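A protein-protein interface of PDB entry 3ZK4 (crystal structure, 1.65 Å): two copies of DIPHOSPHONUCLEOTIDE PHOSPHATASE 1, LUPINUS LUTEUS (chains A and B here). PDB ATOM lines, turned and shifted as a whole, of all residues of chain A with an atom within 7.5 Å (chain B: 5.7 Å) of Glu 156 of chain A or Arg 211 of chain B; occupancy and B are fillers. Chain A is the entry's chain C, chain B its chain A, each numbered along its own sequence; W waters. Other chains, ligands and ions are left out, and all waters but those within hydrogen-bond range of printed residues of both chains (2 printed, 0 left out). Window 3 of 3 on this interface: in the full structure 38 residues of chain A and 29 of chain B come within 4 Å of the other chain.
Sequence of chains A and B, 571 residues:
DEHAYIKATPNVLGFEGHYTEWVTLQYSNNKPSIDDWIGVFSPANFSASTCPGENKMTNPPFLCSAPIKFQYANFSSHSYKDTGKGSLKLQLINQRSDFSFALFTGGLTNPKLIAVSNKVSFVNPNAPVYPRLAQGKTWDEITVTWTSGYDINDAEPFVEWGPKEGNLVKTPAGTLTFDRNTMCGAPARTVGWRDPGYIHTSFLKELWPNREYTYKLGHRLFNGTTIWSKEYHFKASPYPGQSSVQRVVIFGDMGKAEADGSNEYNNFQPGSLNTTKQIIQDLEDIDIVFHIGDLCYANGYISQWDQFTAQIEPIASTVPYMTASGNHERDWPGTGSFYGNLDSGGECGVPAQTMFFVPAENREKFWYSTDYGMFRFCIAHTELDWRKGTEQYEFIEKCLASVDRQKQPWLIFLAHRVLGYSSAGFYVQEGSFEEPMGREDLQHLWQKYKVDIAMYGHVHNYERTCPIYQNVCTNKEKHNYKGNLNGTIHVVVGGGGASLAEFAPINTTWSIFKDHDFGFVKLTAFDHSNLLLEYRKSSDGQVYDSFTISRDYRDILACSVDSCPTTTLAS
NH2 of Arg 211 of chain B lies within salt-bridge range of OE1 of Glu 156 of chain A (3.0 Å).
N of Arg 220 of chain A sits at hydrogen-bond distance from O of Glu 156 of chain A, at 2.9 Å.
The backbone NH of Trp 208 of chain B sits at hydrogen-bond distance from the side-chain hydroxyl of Tyr 213 of chain B, at 2.9 Å.
The backbone carbonyl oxygen of Arg 211 of chain B is in hydrogen-bond range of the backbone NH of Ala 236 of chain B (2.8 Å).
The backbone NH (N) of Asn 210 of chain B is in hydrogen-bond range of the backbone carbonyl oxygen (O) of Ala 236 of chain B, at 3.1 Å.
O of Phe 158 of chain A sits at hydrogen-bond distance from N of Gly 218 of chain A (2.8 Å).
Ile 152 of chain A touches Asn 210 of chain B.
Trp 208 of chain B touches Glu 156 of chain A.
CH2 of Trp 208 of chain B touches CB of Phe 158 of chain A (3.7 Å).
CZ2 of Trp 208 of chain B touches O of Lys 170 of chain A (3.7 Å).
Pro 172 of chain A touches Trp 208 of chain B.
Pro 209 of chain B touches Pro 172 of chain A (CD to CB, 3.7 Å).
O of Ala 173 of chain A touches CG of Pro 209 of chain B, 3.6 Å away.
Of chain B, only Trp 208 (3.5 Å) and Arg 211 (3.0 Å) come within 4 Å of Glu 156 of chain A.
Of the printed residues of chain A, Trp 208 of chain B touches Glu 156, Phe 158, Lys 170 and Pro 172.
Of the printed residues of chain B, Ala 173 of chain A touches Pro 209 (3.6 Å).
The nearest residue of chain B that does not touch Glu 156 of chain A is Pro 209 of chain B (4.4 Å).
Of the 23 printed residues of chain A, 6 touch a printed residue of chain B.
Printed residues of chain A that touch a printed residue of chain B: Ile 152, Glu 156, Phe 158, Lys 170, Pro 172 and Ala 173.
Printed residues of chain B that touch a printed residue of chain A: Trp 208, Pro 209, Asn 210 and Arg 211.
Among the printed residues, 8 pairs touch across the chains.
No position is printed for both chains.
Of the 8 pairs that touch across the chains among the printed residues, none has its exchanged pair printed and touching as well.
Water W1 bridges the backbone carbonyl oxygen (O) of Pro 209 of chain B (2.6 Å) and the side-chain carboxylate (OE2) of Glu 156 of chain A (2.7 Å).
Water W2 lies within hydrogen-bond range of NE1 of Trp 208 of chain B (3.0 Å) and O of Lys 170 of chain A (3.4 Å).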
ATOM      1  N   TRP A 146      11.334  -4.209  19.674  1.00  0.00           N
ATOM      2  CA  TRP A 146      10.396  -5.265  19.201  1.00  0.00           C
ATOM      3  C   TRP A 146       9.154  -4.722  18.576  1.00  0.00           C
ATOM      4  O   TRP A 146       8.918  -3.512  18.566  1.00  0.00           O
ATOM      5  CB  TRP A 146      10.096  -6.218  20.345  1.00  0.00           C
ATOM      6  CG  TRP A 146       9.080  -5.741  21.350  1.00  0.00           C
ATOM      7  CD1 TRP A 146       7.756  -6.080  21.366  1.00  0.00           C
ATOM      8  CD2 TRP A 146       9.307  -4.907  22.526  1.00  0.00           C
ATOM      9  NE1 TRP A 146       7.131  -5.489  22.474  1.00  0.00           N
ATOM     10  CE2 TRP A 146       8.052  -4.757  23.181  1.00  0.00           C
ATOM     11  CE3 TRP A 146      10.428  -4.214  23.040  1.00  0.00           C
ATOM     12  CZ2 TRP A 146       7.899  -4.011  24.350  1.00  0.00           C
ATOM     13  CZ3 TRP A 146      10.268  -3.438  24.206  1.00  0.00           C
ATOM     14  CH2 TRP A 146       9.017  -3.372  24.868  1.00  0.00           C
ATOM     15  N   TYR A 150       0.063  -3.735  19.709  1.00  0.00           N
ATOM     16  CA  TYR A 150      -0.534  -2.918  20.798  1.00  0.00           C
ATOM     17  C   TYR A 150      -0.030  -1.465  20.789  1.00  0.00           C
ATOM     18  O   TYR A 150       1.133  -1.230  21.149  1.00  0.00           O
ATOM     19  CB  TYR A 150      -0.177  -3.538  22.133  1.00  0.00           C
ATOM     20  CG  TYR A 150      -0.731  -4.938  22.347  1.00  0.00           C
ATOM     21  CD1 TYR A 150      -2.091  -5.150  22.456  1.00  0.00           C
ATOM     22  CD2 TYR A 150       0.113  -5.999  22.525  1.00  0.00           C
ATOM     23  CE1 TYR A 150      -2.585  -6.431  22.684  1.00  0.00           C
ATOM     24  CE2 TYR A 150      -0.361  -7.290  22.717  1.00  0.00           C
ATOM     25  CZ  TYR A 150      -1.719  -7.487  22.830  1.00  0.00           C
ATOM     26  OH  TYR A 150      -2.155  -8.792  23.043  1.00  0.00           O
ATOM     27  N   ASP A 151      -0.900  -0.536  20.401  1.00  0.00           N
ATOM     28  CA  ASP A 151      -0.632   0.908  20.518  1.00  0.00           C
ATOM     29  C   ASP A 151      -0.629   1.304  21.994  1.00  0.00           C
ATOM     30  O   ASP A 151      -1.015   0.520  22.861  1.00  0.00           O
ATOM     31  CB  ASP A 151      -1.630   1.746  19.742  1.00  0.00           C
ATOM     32  CG  ASP A 151      -1.040   3.118  19.304  1.00  0.00           C
ATOM     33  OD1 ASP A 151       0.102   3.473  19.737  1.00  0.00           O
ATOM     34  OD2 ASP A 151      -1.719   3.818  18.524  1.00  0.00           O
ATOM     35  N   ILE A 152      -0.139   2.508  22.283  1.00  0.00           N
ATOM     36  CA  ILE A 152       0.019   2.941  23.660  1.00  0.00           C
ATOM     37  C   ILE A 152      -1.315   3.125  24.390  1.00  0.00           C
ATOM     38  O   ILE A 152      -1.326   3.041  25.589  1.00  0.00           O
ATOM     39  CB  ILE A 152       0.828   4.241  23.774  1.00  0.00           C
ATOM     40  CG1 ILE A 152       0.180   5.360  22.990  1.00  0.00           C
ATOM     41  CG2 ILE A 152       2.240   3.988  23.273  1.00  0.00           C
ATOM     42  CD1 ILE A 152       0.902   6.708  23.165  1.00  0.00           C
ATOM     43  N   ASN A 153      -2.385   3.332  23.645  1.00  0.00           N
ATOM     44  CA  ASN A 153      -3.736   3.385  24.231  1.00  0.00           C
ATOM     45  C   ASN A 153      -4.332   1.969  24.451  1.00  0.00           C
ATOM     46  O   ASN A 153      -5.295   1.829  25.181  1.00  0.00           O
ATOM     47  CB  ASN A 153      -4.641   4.256  23.357  1.00  0.00           C
ATOM     48  CG  ASN A 153      -4.790   3.724  21.937  1.00  0.00           C
ATOM     49  OD1 ASN A 153      -3.814   3.371  21.278  1.00  0.00           O
ATOM     50  ND2 ASN A 153      -6.019   3.689  21.450  1.00  0.00           N
ATOM     51  N   ASP A 154      -3.745   0.940  23.842  1.00  0.00           N
ATOM     52  CA  ASP A 154      -4.169  -0.477  24.046  1.00  0.00           C
ATOM     53  C   ASP A 154      -3.444  -1.127  25.235  1.00  0.00           C
ATOM     54  O   ASP A 154      -4.019  -1.941  25.976  1.00  0.00           O
ATOM     55  CB  ASP A 154      -3.875  -1.339  22.799  1.00  0.00           C
ATOM     56  CG  ASP A 154      -4.504  -0.808  21.517  1.00  0.00           C
ATOM     57  OD1 ASP A 154      -5.686  -0.369  21.535  1.00  0.00           O
ATOM     58  OD2 ASP A 154      -3.808  -0.874  20.461  1.00  0.00           O
ATOM     59  N   ALA A 155      -2.159  -0.785  25.441  1.00  0.00           N
ATOM     60  CA  ALA A 155      -1.341  -1.400  26.468  1.00  0.00           C
ATOM     61  C   ALA A 155      -0.101  -0.541  26.704  1.00  0.00           C
ATOM     62  O   ALA A 155       0.375   0.067  25.778  1.00  0.00           O
ATOM     63  CB  ALA A 155      -0.884  -2.784  26.060  1.00  0.00           C
ATOM     64  N   GLU A 156       0.430  -0.586  27.910  1.00  0.00           N
ATOM     65  CA  GLU A 156       1.678   0.065  28.230  1.00  0.00           C
ATOM     66  C   GLU A 156       2.790  -0.936  28.008  1.00  0.00           C
ATOM     67  O   GLU A 156       2.876  -1.974  28.687  1.00  0.00           O
ATOM     68  CB  GLU A 156       1.698   0.556  29.675  1.00  0.00           C
ATOM     69  CG  GLU A 156       2.928   1.432  29.989  1.00  0.00           C
ATOM     70  CD  GLU A 156       2.835   2.096  31.341  1.00  0.00           C
ATOM     71  OE1 GLU A 156       2.527   1.372  32.312  1.00  0.00           O
ATOM     72  OE2 GLU A 156       3.155   3.301  31.491  1.00  0.00           O
ATOM     73  N   PRO A 157       3.691  -0.636  27.050  1.00  0.00           N
ATOM     74  CA  PRO A 157       4.772  -1.576  26.751  1.00  0.00           C
ATOM     75  C   PRO A 157       5.894  -1.460  27.753  1.00  0.00           C
ATOM     76  O   PRO A 157       6.124  -0.369  28.317  1.00  0.00           O
ATOM     77  CB  PRO A 157       5.237  -1.118  25.366  1.00  0.00           C
ATOM     78  CG  PRO A 157       5.029   0.390  25.394  1.00  0.00           C
ATOM     79  CD  PRO A 157       3.734   0.556  26.182  1.00  0.00           C
ATOM     80  N   PHE A 158       6.619  -2.539  27.983  1.00  0.00           N
ATOM     81  CA  PHE A 158       7.756  -2.514  28.886  1.00  0.00           C
ATOM     82  C   PHE A 158       8.611  -3.748  28.661  1.00  0.00           C
ATOM     83  O   PHE A 158       8.199  -4.702  27.975  1.00  0.00           O
ATOM     84  CB  PHE A 158       7.353  -2.410  30.363  1.00  0.00           C
ATOM     85  CG  PHE A 158       6.619  -3.639  30.865  1.00  0.00           C
ATOM     86  CD1 PHE A 158       5.262  -3.756  30.643  1.00  0.00           C
ATOM     87  CD2 PHE A 158       7.290  -4.663  31.520  1.00  0.00           C
ATOM     88  CE1 PHE A 158       4.576  -4.886  31.089  1.00  0.00           C
ATOM     89  CE2 PHE A 158       6.612  -5.806  31.956  1.00  0.00           C
ATOM     90  CZ  PHE A 158       5.248  -5.884  31.763  1.00  0.00           C
ATOM     91  N   VAL A 159       9.805  -3.713  29.238  1.00  0.00           N
ATOM     92  CA  VAL A 159      10.675  -4.865  29.285  1.00  0.00           C
ATOM     93  C   VAL A 159      10.912  -5.177  30.722  1.00  0.00           C
ATOM     94  O   VAL A 159      11.172  -4.281  31.536  1.00  0.00           O
ATOM     95  CB  VAL A 159      12.031  -4.659  28.523  1.00  0.00           C
ATOM     96  CG1 VAL A 159      13.048  -5.699  28.922  1.00  0.00           C
ATOM     97  CG2 VAL A 159      11.785  -4.716  27.041  1.00  0.00           C
ATOM     98  N   LYS A 170      11.118  -3.684  35.829  1.00  0.00           N
ATOM     99  CA  LYS A 170      10.451  -3.273  34.622  1.00  0.00           C
ATOM    100  C   LYS A 170      10.993  -1.915  34.189  1.00  0.00           C
ATOM    101  O   LYS A 170      11.214  -1.056  35.025  1.00  0.00           O
ATOM    102  CB  LYS A 170       8.949  -3.153  34.849  1.00  0.00           C
ATOM    103  CG  LYS A 170       8.262  -4.457  35.276  1.00  0.00           C
ATOM    104  CD  LYS A 170       6.759  -4.297  35.163  1.00  0.00           C
ATOM    105  CE  LYS A 170       5.998  -5.576  35.488  1.00  0.00           C
ATOM    106  NZ  LYS A 170       6.111  -5.924  36.913  1.00  0.00           N
ATOM    107  N   PRO A 172      10.472   1.162  30.905  1.00  0.00           N
ATOM    108  CA  PRO A 172       9.520   1.560  29.890  1.00  0.00           C
ATOM    109  C   PRO A 172      10.019   1.307  28.501  1.00  0.00           C
ATOM    110  O   PRO A 172      11.195   0.981  28.317  1.00  0.00           O
ATOM    111  CB  PRO A 172       9.366   3.081  30.113  1.00  0.00           C
ATOM    112  CG  PRO A 172      10.615   3.492  30.828  1.00  0.00           C
ATOM    113  CD  PRO A 172      11.025   2.312  31.651  1.00  0.00           C
ATOM    114  N   ALA A 173       9.162   1.573  27.532  1.00  0.00           N
ATOM    115  CA  ALA A 173       9.561   1.561  26.152  1.00  0.00           C
ATOM    116  C   ALA A 173       8.978   2.759  25.462  1.00  0.00           C
ATOM    117  O   ALA A 173       7.898   3.213  25.781  1.00  0.00           O
ATOM    118  CB  ALA A 173       9.110   0.271  25.493  1.00  0.00           C
ATOM    119  N   THR A 175       7.432   4.101  21.963  1.00  0.00           N
ATOM    120  CA  THR A 175       6.687   3.465  20.895  1.00  0.00           C
ATOM    121  C   THR A 175       6.600   4.347  19.698  1.00  0.00           C
ATOM    122  O   THR A 175       6.187   5.504  19.800  1.00  0.00           O
ATOM    123  CB  THR A 175       5.255   3.118  21.405  1.00  0.00           C
ATOM    124  OG1 THR A 175       5.368   2.219  22.502  1.00  0.00           O
ATOM    125  CG2 THR A 175       4.355   2.508  20.273  1.00  0.00           C
ATOM    126  N   HIS A 200       8.572  -0.837  19.538  1.00  0.00           N
ATOM    127  CA  HIS A 200       8.846  -0.453  20.925  1.00  0.00           C
ATOM    128  C   HIS A 200      10.313  -0.613  21.186  1.00  0.00           C
ATOM    129  O   HIS A 200      10.894  -1.620  20.818  1.00  0.00           O
ATOM    130  CB  HIS A 200       8.095  -1.327  21.932  1.00  0.00           C
ATOM    131  CG  HIS A 200       6.666  -1.523  21.581  1.00  0.00           C
ATOM    132  ND1 HIS A 200       5.708  -0.550  21.738  1.00  0.00           N
ATOM    133  CD2 HIS A 200       6.032  -2.593  21.039  1.00  0.00           C
ATOM    134  CE1 HIS A 200       4.538  -1.011  21.316  1.00  0.00           C
ATOM    135  NE2 HIS A 200       4.718  -2.242  20.864  1.00  0.00           N
ATOM    136  N   GLY A 218       6.816  -7.131  27.438  1.00  0.00           N
ATOM    137  CA  GLY A 218       5.490  -7.071  28.128  1.00  0.00           C
ATOM    138  C   GLY A 218       4.604  -5.946  27.681  1.00  0.00           C
ATOM    139  O   GLY A 218       5.096  -4.860  27.274  1.00  0.00           O
ATOM    140  N   HIS A 219       3.282  -6.188  27.658  1.00  0.00           N
ATOM    141  CA  HIS A 219       2.289  -5.183  27.365  1.00  0.00           C
ATOM    142  C   HIS A 219       1.223  -5.248  28.439  1.00  0.00           C
ATOM    143  O   HIS A 219       0.542  -6.272  28.524  1.00  0.00           O
ATOM    144  CB  HIS A 219       1.700  -5.444  25.992  1.00  0.00           C
ATOM    145  CG  HIS A 219       2.731  -5.337  24.926  1.00  0.00           C
ATOM    146  ND1 HIS A 219       2.990  -4.146  24.278  1.00  0.00           N
ATOM    147  CD2 HIS A 219       3.690  -6.203  24.523  1.00  0.00           C
ATOM    148  CE1 HIS A 219       3.993  -4.319  23.433  1.00  0.00           C
ATOM    149  NE2 HIS A 219       4.455  -5.546  23.578  1.00  0.00           N
ATOM    150  N   ARG A 220       1.101  -4.204  29.263  1.00  0.00           N
ATOM    151  CA  ARG A 220       0.044  -4.193  30.278  1.00  0.00           C
ATOM    152  C   ARG A 220      -1.213  -3.608  29.667  1.00  0.00           C
ATOM    153  O   ARG A 220      -1.319  -2.426  29.430  1.00  0.00           O
ATOM    154  CB  ARG A 220       0.469  -3.486  31.570  1.00  0.00           C
ATOM    155  CG  ARG A 220      -0.483  -3.772  32.741  1.00  0.00           C
ATOM    156  CD  ARG A 220      -0.199  -2.958  33.998  1.00  0.00           C
ATOM    157  NE  ARG A 220      -1.395  -2.889  34.852  1.00  0.00           N
ATOM    158  CZ  ARG A 220      -2.404  -2.022  34.690  1.00  0.00           C
ATOM    159  NH1 ARG A 220      -2.383  -1.095  33.728  1.00  0.00           N
ATOM    160  NH2 ARG A 220      -3.443  -2.066  35.518  1.00  0.00           N
ATOM    161  N   LEU A 221      -2.186  -4.480  29.392  1.00  0.00           N
ATOM    162  CA  LEU A 221      -3.432  -4.042  28.833  1.00  0.00           C
ATOM    163  C   LEU A 221      -4.166  -3.182  29.855  1.00  0.00           C
ATOM    164  O   LEU A 221      -4.005  -3.345  31.053  1.00  0.00           O
ATOM    165  CB  LEU A 221      -4.294  -5.241  28.466  1.00  0.00           C
ATOM    166  CG  LEU A 221      -3.670  -6.285  27.540  1.00  0.00           C
ATOM    167  CD1 LEU A 221      -4.635  -7.479  27.394  1.00  0.00           C
ATOM    168  CD2 LEU A 221      -3.422  -5.708  26.179  1.00  0.00           C
ATOM    169  N   PHE A 222      -4.967  -2.261  29.383  1.00  0.00           N
ATOM    170  CA  PHE A 222      -5.618  -1.370  30.331  1.00  0.00           C
ATOM    171  C   PHE A 222      -6.743  -2.064  31.095  1.00  0.00           C
ATOM    172  O   PHE A 222      -7.096  -1.610  32.165  1.00  0.00           O
ATOM    173  CB  PHE A 222      -6.013  -0.059  29.670  1.00  0.00           C
ATOM    174  CG  PHE A 222      -4.802   0.786  29.313  1.00  0.00           C
ATOM    175  CD1 PHE A 222      -4.020   1.365  30.310  1.00  0.00           C
ATOM    176  CD2 PHE A 222      -4.410   0.952  27.993  1.00  0.00           C
ATOM    177  CE1 PHE A 222      -2.898   2.120  29.984  1.00  0.00           C
ATOM    178  CE2 PHE A 222      -3.294   1.711  27.668  1.00  0.00           C
ATOM    179  CZ  PHE A 222      -2.536   2.293  28.659  1.00  0.00           C
ATOM    180  N   THR A 226      -1.511  -8.552  31.753  1.00  0.00           N
ATOM    181  CA  THR A 226      -0.240  -8.333  31.048  1.00  0.00           C
ATOM    182  C   THR A 226       0.006  -9.475  30.075  1.00  0.00           C
ATOM    183  O   THR A 226      -0.108 -10.664  30.451  1.00  0.00           O
ATOM    184  CB  THR A 226       0.907  -8.204  32.035  1.00  0.00           C
ATOM    185  OG1 THR A 226       0.671  -7.039  32.852  1.00  0.00           O
ATOM    186  CG2 THR A 226       2.262  -8.078  31.308  1.00  0.00           C
ATOM    187  N   ILE A 227       0.291  -9.100  28.825  1.00  0.00           N
ATOM    188  CA  ILE A 227       0.693 -10.045  27.783  1.00  0.00           C
ATOM    189  C   ILE A 227       2.227 -10.108  27.748  1.00  0.00           C
ATOM    190  O   ILE A 227       2.884  -9.052  27.678  1.00  0.00           O
ATOM    191  CB  ILE A 227       0.134  -9.607  26.425  1.00  0.00           C
ATOM    192  CG1 ILE A 227      -1.394  -9.508  26.486  1.00  0.00           C
ATOM    193  CG2 ILE A 227       0.635 -10.547  25.322  1.00  0.00           C
ATOM    194  CD1 ILE A 227      -2.078 -10.789  26.960  1.00  0.00           C
ATOM    195  N   PRO B 163       5.107   6.982  40.528  1.00  0.00           N
ATOM    196  CA  PRO B 163       3.886   6.828  39.772  1.00  0.00           C
ATOM    197  C   PRO B 163       2.702   6.990  40.686  1.00  0.00           C
ATOM    198  O   PRO B 163       2.800   6.686  41.893  1.00  0.00           O
ATOM    199  CB  PRO B 163       3.955   5.390  39.236  1.00  0.00           C
ATOM    200  CG  PRO B 163       5.334   4.944  39.471  1.00  0.00           C
ATOM    201  CD  PRO B 163       5.901   5.746  40.599  1.00  0.00           C
ATOM    202  N   TRP B 208       8.593   6.967  32.653  1.00  0.00           N
ATOM    203  CA  TRP B 208       7.837   6.264  31.663  1.00  0.00           C
ATOM    204  C   TRP B 208       6.995   7.231  30.885  1.00  0.00           C
ATOM    205  O   TRP B 208       6.240   8.022  31.472  1.00  0.00           O
ATOM    206  CB  TRP B 208       6.919   5.231  32.351  1.00  0.00           C
ATOM    207  CG  TRP B 208       7.598   4.129  33.097  1.00  0.00           C
ATOM    208  CD1 TRP B 208       8.556   4.214  34.026  1.00  0.00           C
ATOM    209  CD2 TRP B 208       7.264   2.725  32.992  1.00  0.00           C
ATOM    210  NE1 TRP B 208       8.890   2.960  34.506  1.00  0.00           N
ATOM    211  CE2 TRP B 208       8.105   2.032  33.865  1.00  0.00           C
ATOM    212  CE3 TRP B 208       6.360   2.006  32.208  1.00  0.00           C
ATOM    213  CZ2 TRP B 208       8.063   0.601  34.002  1.00  0.00           C
ATOM    214  CZ3 TRP B 208       6.326   0.614  32.323  1.00  0.00           C
ATOM    215  CH2 TRP B 208       7.165  -0.061  33.224  1.00  0.00           C
ATOM    216  N   PRO B 209       7.075   7.176  29.553  1.00  0.00           N
ATOM    217  CA  PRO B 209       6.351   8.134  28.775  1.00  0.00           C
ATOM    218  C   PRO B 209       4.825   7.997  29.024  1.00  0.00           C
ATOM    219  O   PRO B 209       4.330   6.879  29.177  1.00  0.00           O
ATOM    220  CB  PRO B 209       6.723   7.794  27.345  1.00  0.00           C
ATOM    221  CG  PRO B 209       7.185   6.366  27.380  1.00  0.00           C
ATOM    222  CD  PRO B 209       7.784   6.161  28.730  1.00  0.00           C
ATOM    223  N   ASN B 210       4.135   9.139  29.122  1.00  0.00           N
ATOM    224  CA  ASN B 210       2.696   9.185  29.267  1.00  0.00           C
ATOM    225  C   ASN B 210       2.161   8.760  30.621  1.00  0.00           C
ATOM    226  O   ASN B 210       0.924   8.753  30.805  1.00  0.00           O
ATOM    227  CB  ASN B 210       2.009   8.358  28.182  1.00  0.00           C
ATOM    228  CG  ASN B 210       2.615   8.574  26.818  1.00  0.00           C
ATOM    229  OD1 ASN B 210       2.643   9.696  26.331  1.00  0.00           O
ATOM    230  ND2 ASN B 210       3.137   7.508  26.224  1.00  0.00           N
ATOM    231  N   ARG B 211       3.027   8.393  31.534  1.00  0.00           N
ATOM    232  CA  ARG B 211       2.581   7.883  32.825  1.00  0.00           C
ATOM    233  C   ARG B 211       2.288   9.025  33.781  1.00  0.00           C
ATOM    234  O   ARG B 211       2.919  10.088  33.742  1.00  0.00           O
ATOM    235  CB  ARG B 211       3.652   6.967  33.385  1.00  0.00           C
ATOM    236  CG  ARG B 211       3.351   6.363  34.718  1.00  0.00           C
ATOM    237  CD  ARG B 211       4.444   5.388  35.136  1.00  0.00           C
ATOM    238  NE  ARG B 211       4.151   4.055  34.661  1.00  0.00           N
ATOM    239  CZ  ARG B 211       4.660   2.924  35.184  1.00  0.00           C
ATOM    240  NH1 ARG B 211       5.512   2.966  36.188  1.00  0.00           N
ATOM    241  NH2 ARG B 211       4.298   1.738  34.689  1.00  0.00           N
ATOM    242  N   GLU B 212       1.319   8.784  34.648  1.00  0.00           N
ATOM    243  CA  GLU B 212       0.907   9.733  35.656  1.00  0.00           C
ATOM    244  C   GLU B 212       1.742   9.586  36.896  1.00  0.00           C
ATOM    245  O   GLU B 212       1.966   8.467  37.423  1.00  0.00           O
ATOM    246  CB  GLU B 212      -0.561   9.497  36.035  1.00  0.00           C
ATOM    247  CG  GLU B 212      -1.510   9.876  34.930  1.00  0.00           C
ATOM    248  CD  GLU B 212      -1.671  11.353  34.767  1.00  0.00           C
ATOM    249  OE1 GLU B 212      -1.274  12.136  35.670  1.00  0.00           O
ATOM    250  OE2 GLU B 212      -2.248  11.737  33.745  1.00  0.00           O
ATOM    251  N   TYR B 213       2.242  10.729  37.387  1.00  0.00           N
ATOM    252  CA  TYR B 213       3.101  10.785  38.535  1.00  0.00           C
ATOM    253  C   TYR B 213       2.586  11.769  39.594  1.00  0.00           C
ATOM    254  O   TYR B 213       1.858  12.698  39.287  1.00  0.00           O
ATOM    255  CB  TYR B 213       4.543  11.246  38.108  1.00  0.00           C
ATOM    256  CG  TYR B 213       5.337  10.195  37.343  1.00  0.00           C
ATOM    257  CD1 TYR B 213       6.113   9.254  38.006  1.00  0.00           C
ATOM    258  CD2 TYR B 213       5.304  10.158  35.973  1.00  0.00           C
ATOM    259  CE1 TYR B 213       6.797   8.285  37.345  1.00  0.00           C
ATOM    260  CE2 TYR B 213       6.022   9.193  35.293  1.00  0.00           C
ATOM    261  CZ  TYR B 213       6.736   8.255  35.972  1.00  0.00           C
ATOM    262  OH  TYR B 213       7.439   7.258  35.312  1.00  0.00           O
ATOM    263  N   PHE B 234       1.776  15.316  37.727  1.00  0.00           N
ATOM    264  CA  PHE B 234       2.015  15.565  36.314  1.00  0.00           C
ATOM    265  C   PHE B 234       1.946  14.272  35.534  1.00  0.00           C
ATOM    266  O   PHE B 234       2.070  13.192  36.106  1.00  0.00           O
ATOM    267  CB  PHE B 234       3.398  16.251  36.047  1.00  0.00           C
ATOM    268  CG  PHE B 234       4.580  15.386  36.369  1.00  0.00           C
ATOM    269  CD1 PHE B 234       5.115  15.340  37.655  1.00  0.00           C
ATOM    270  CD2 PHE B 234       5.203  14.640  35.380  1.00  0.00           C
ATOM    271  CE1 PHE B 234       6.197  14.560  37.955  1.00  0.00           C
ATOM    272  CE2 PHE B 234       6.289  13.817  35.686  1.00  0.00           C
ATOM    273  CZ  PHE B 234       6.794  13.779  36.981  1.00  0.00           C
ATOM    274  N   LYS B 235       1.777  14.435  34.236  1.00  0.00           N
ATOM    275  CA  LYS B 235       1.834  13.341  33.269  1.00  0.00           C
ATOM    276  C   LYS B 235       3.177  13.478  32.494  1.00  0.00           C
ATOM    277  O   LYS B 235       3.477  14.563  31.973  1.00  0.00           O
ATOM    278  CB  LYS B 235       0.684  13.418  32.299  1.00  0.00           C
ATOM    279  CG  LYS B 235       0.649  12.248  31.338  1.00  0.00           C
ATOM    280  CD  LYS B 235      -0.535  12.425  30.395  1.00  0.00           C
ATOM    281  CE  LYS B 235      -0.624  11.253  29.442  1.00  0.00           C
ATOM    282  NZ  LYS B 235      -1.753  11.457  28.514  1.00  0.00           N
ATOM    283  N   ALA B 236       3.965  12.415  32.497  1.00  0.00           N
ATOM    284  CA  ALA B 236       5.250  12.422  31.756  1.00  0.00           C
ATOM    285  C   ALA B 236       5.052  12.658  30.277  1.00  0.00           C
ATOM    286  O   ALA B 236       4.098  12.232  29.664  1.00  0.00           O
ATOM    287  CB  ALA B 236       6.051  11.167  31.987  1.00  0.00           C
HETATM  288  O   HOH W   1       4.575   4.288  29.381  1.00  0.00           O
HETATM  289  O   HOH W   2      10.534   1.777  36.688  1.00  0.00           O
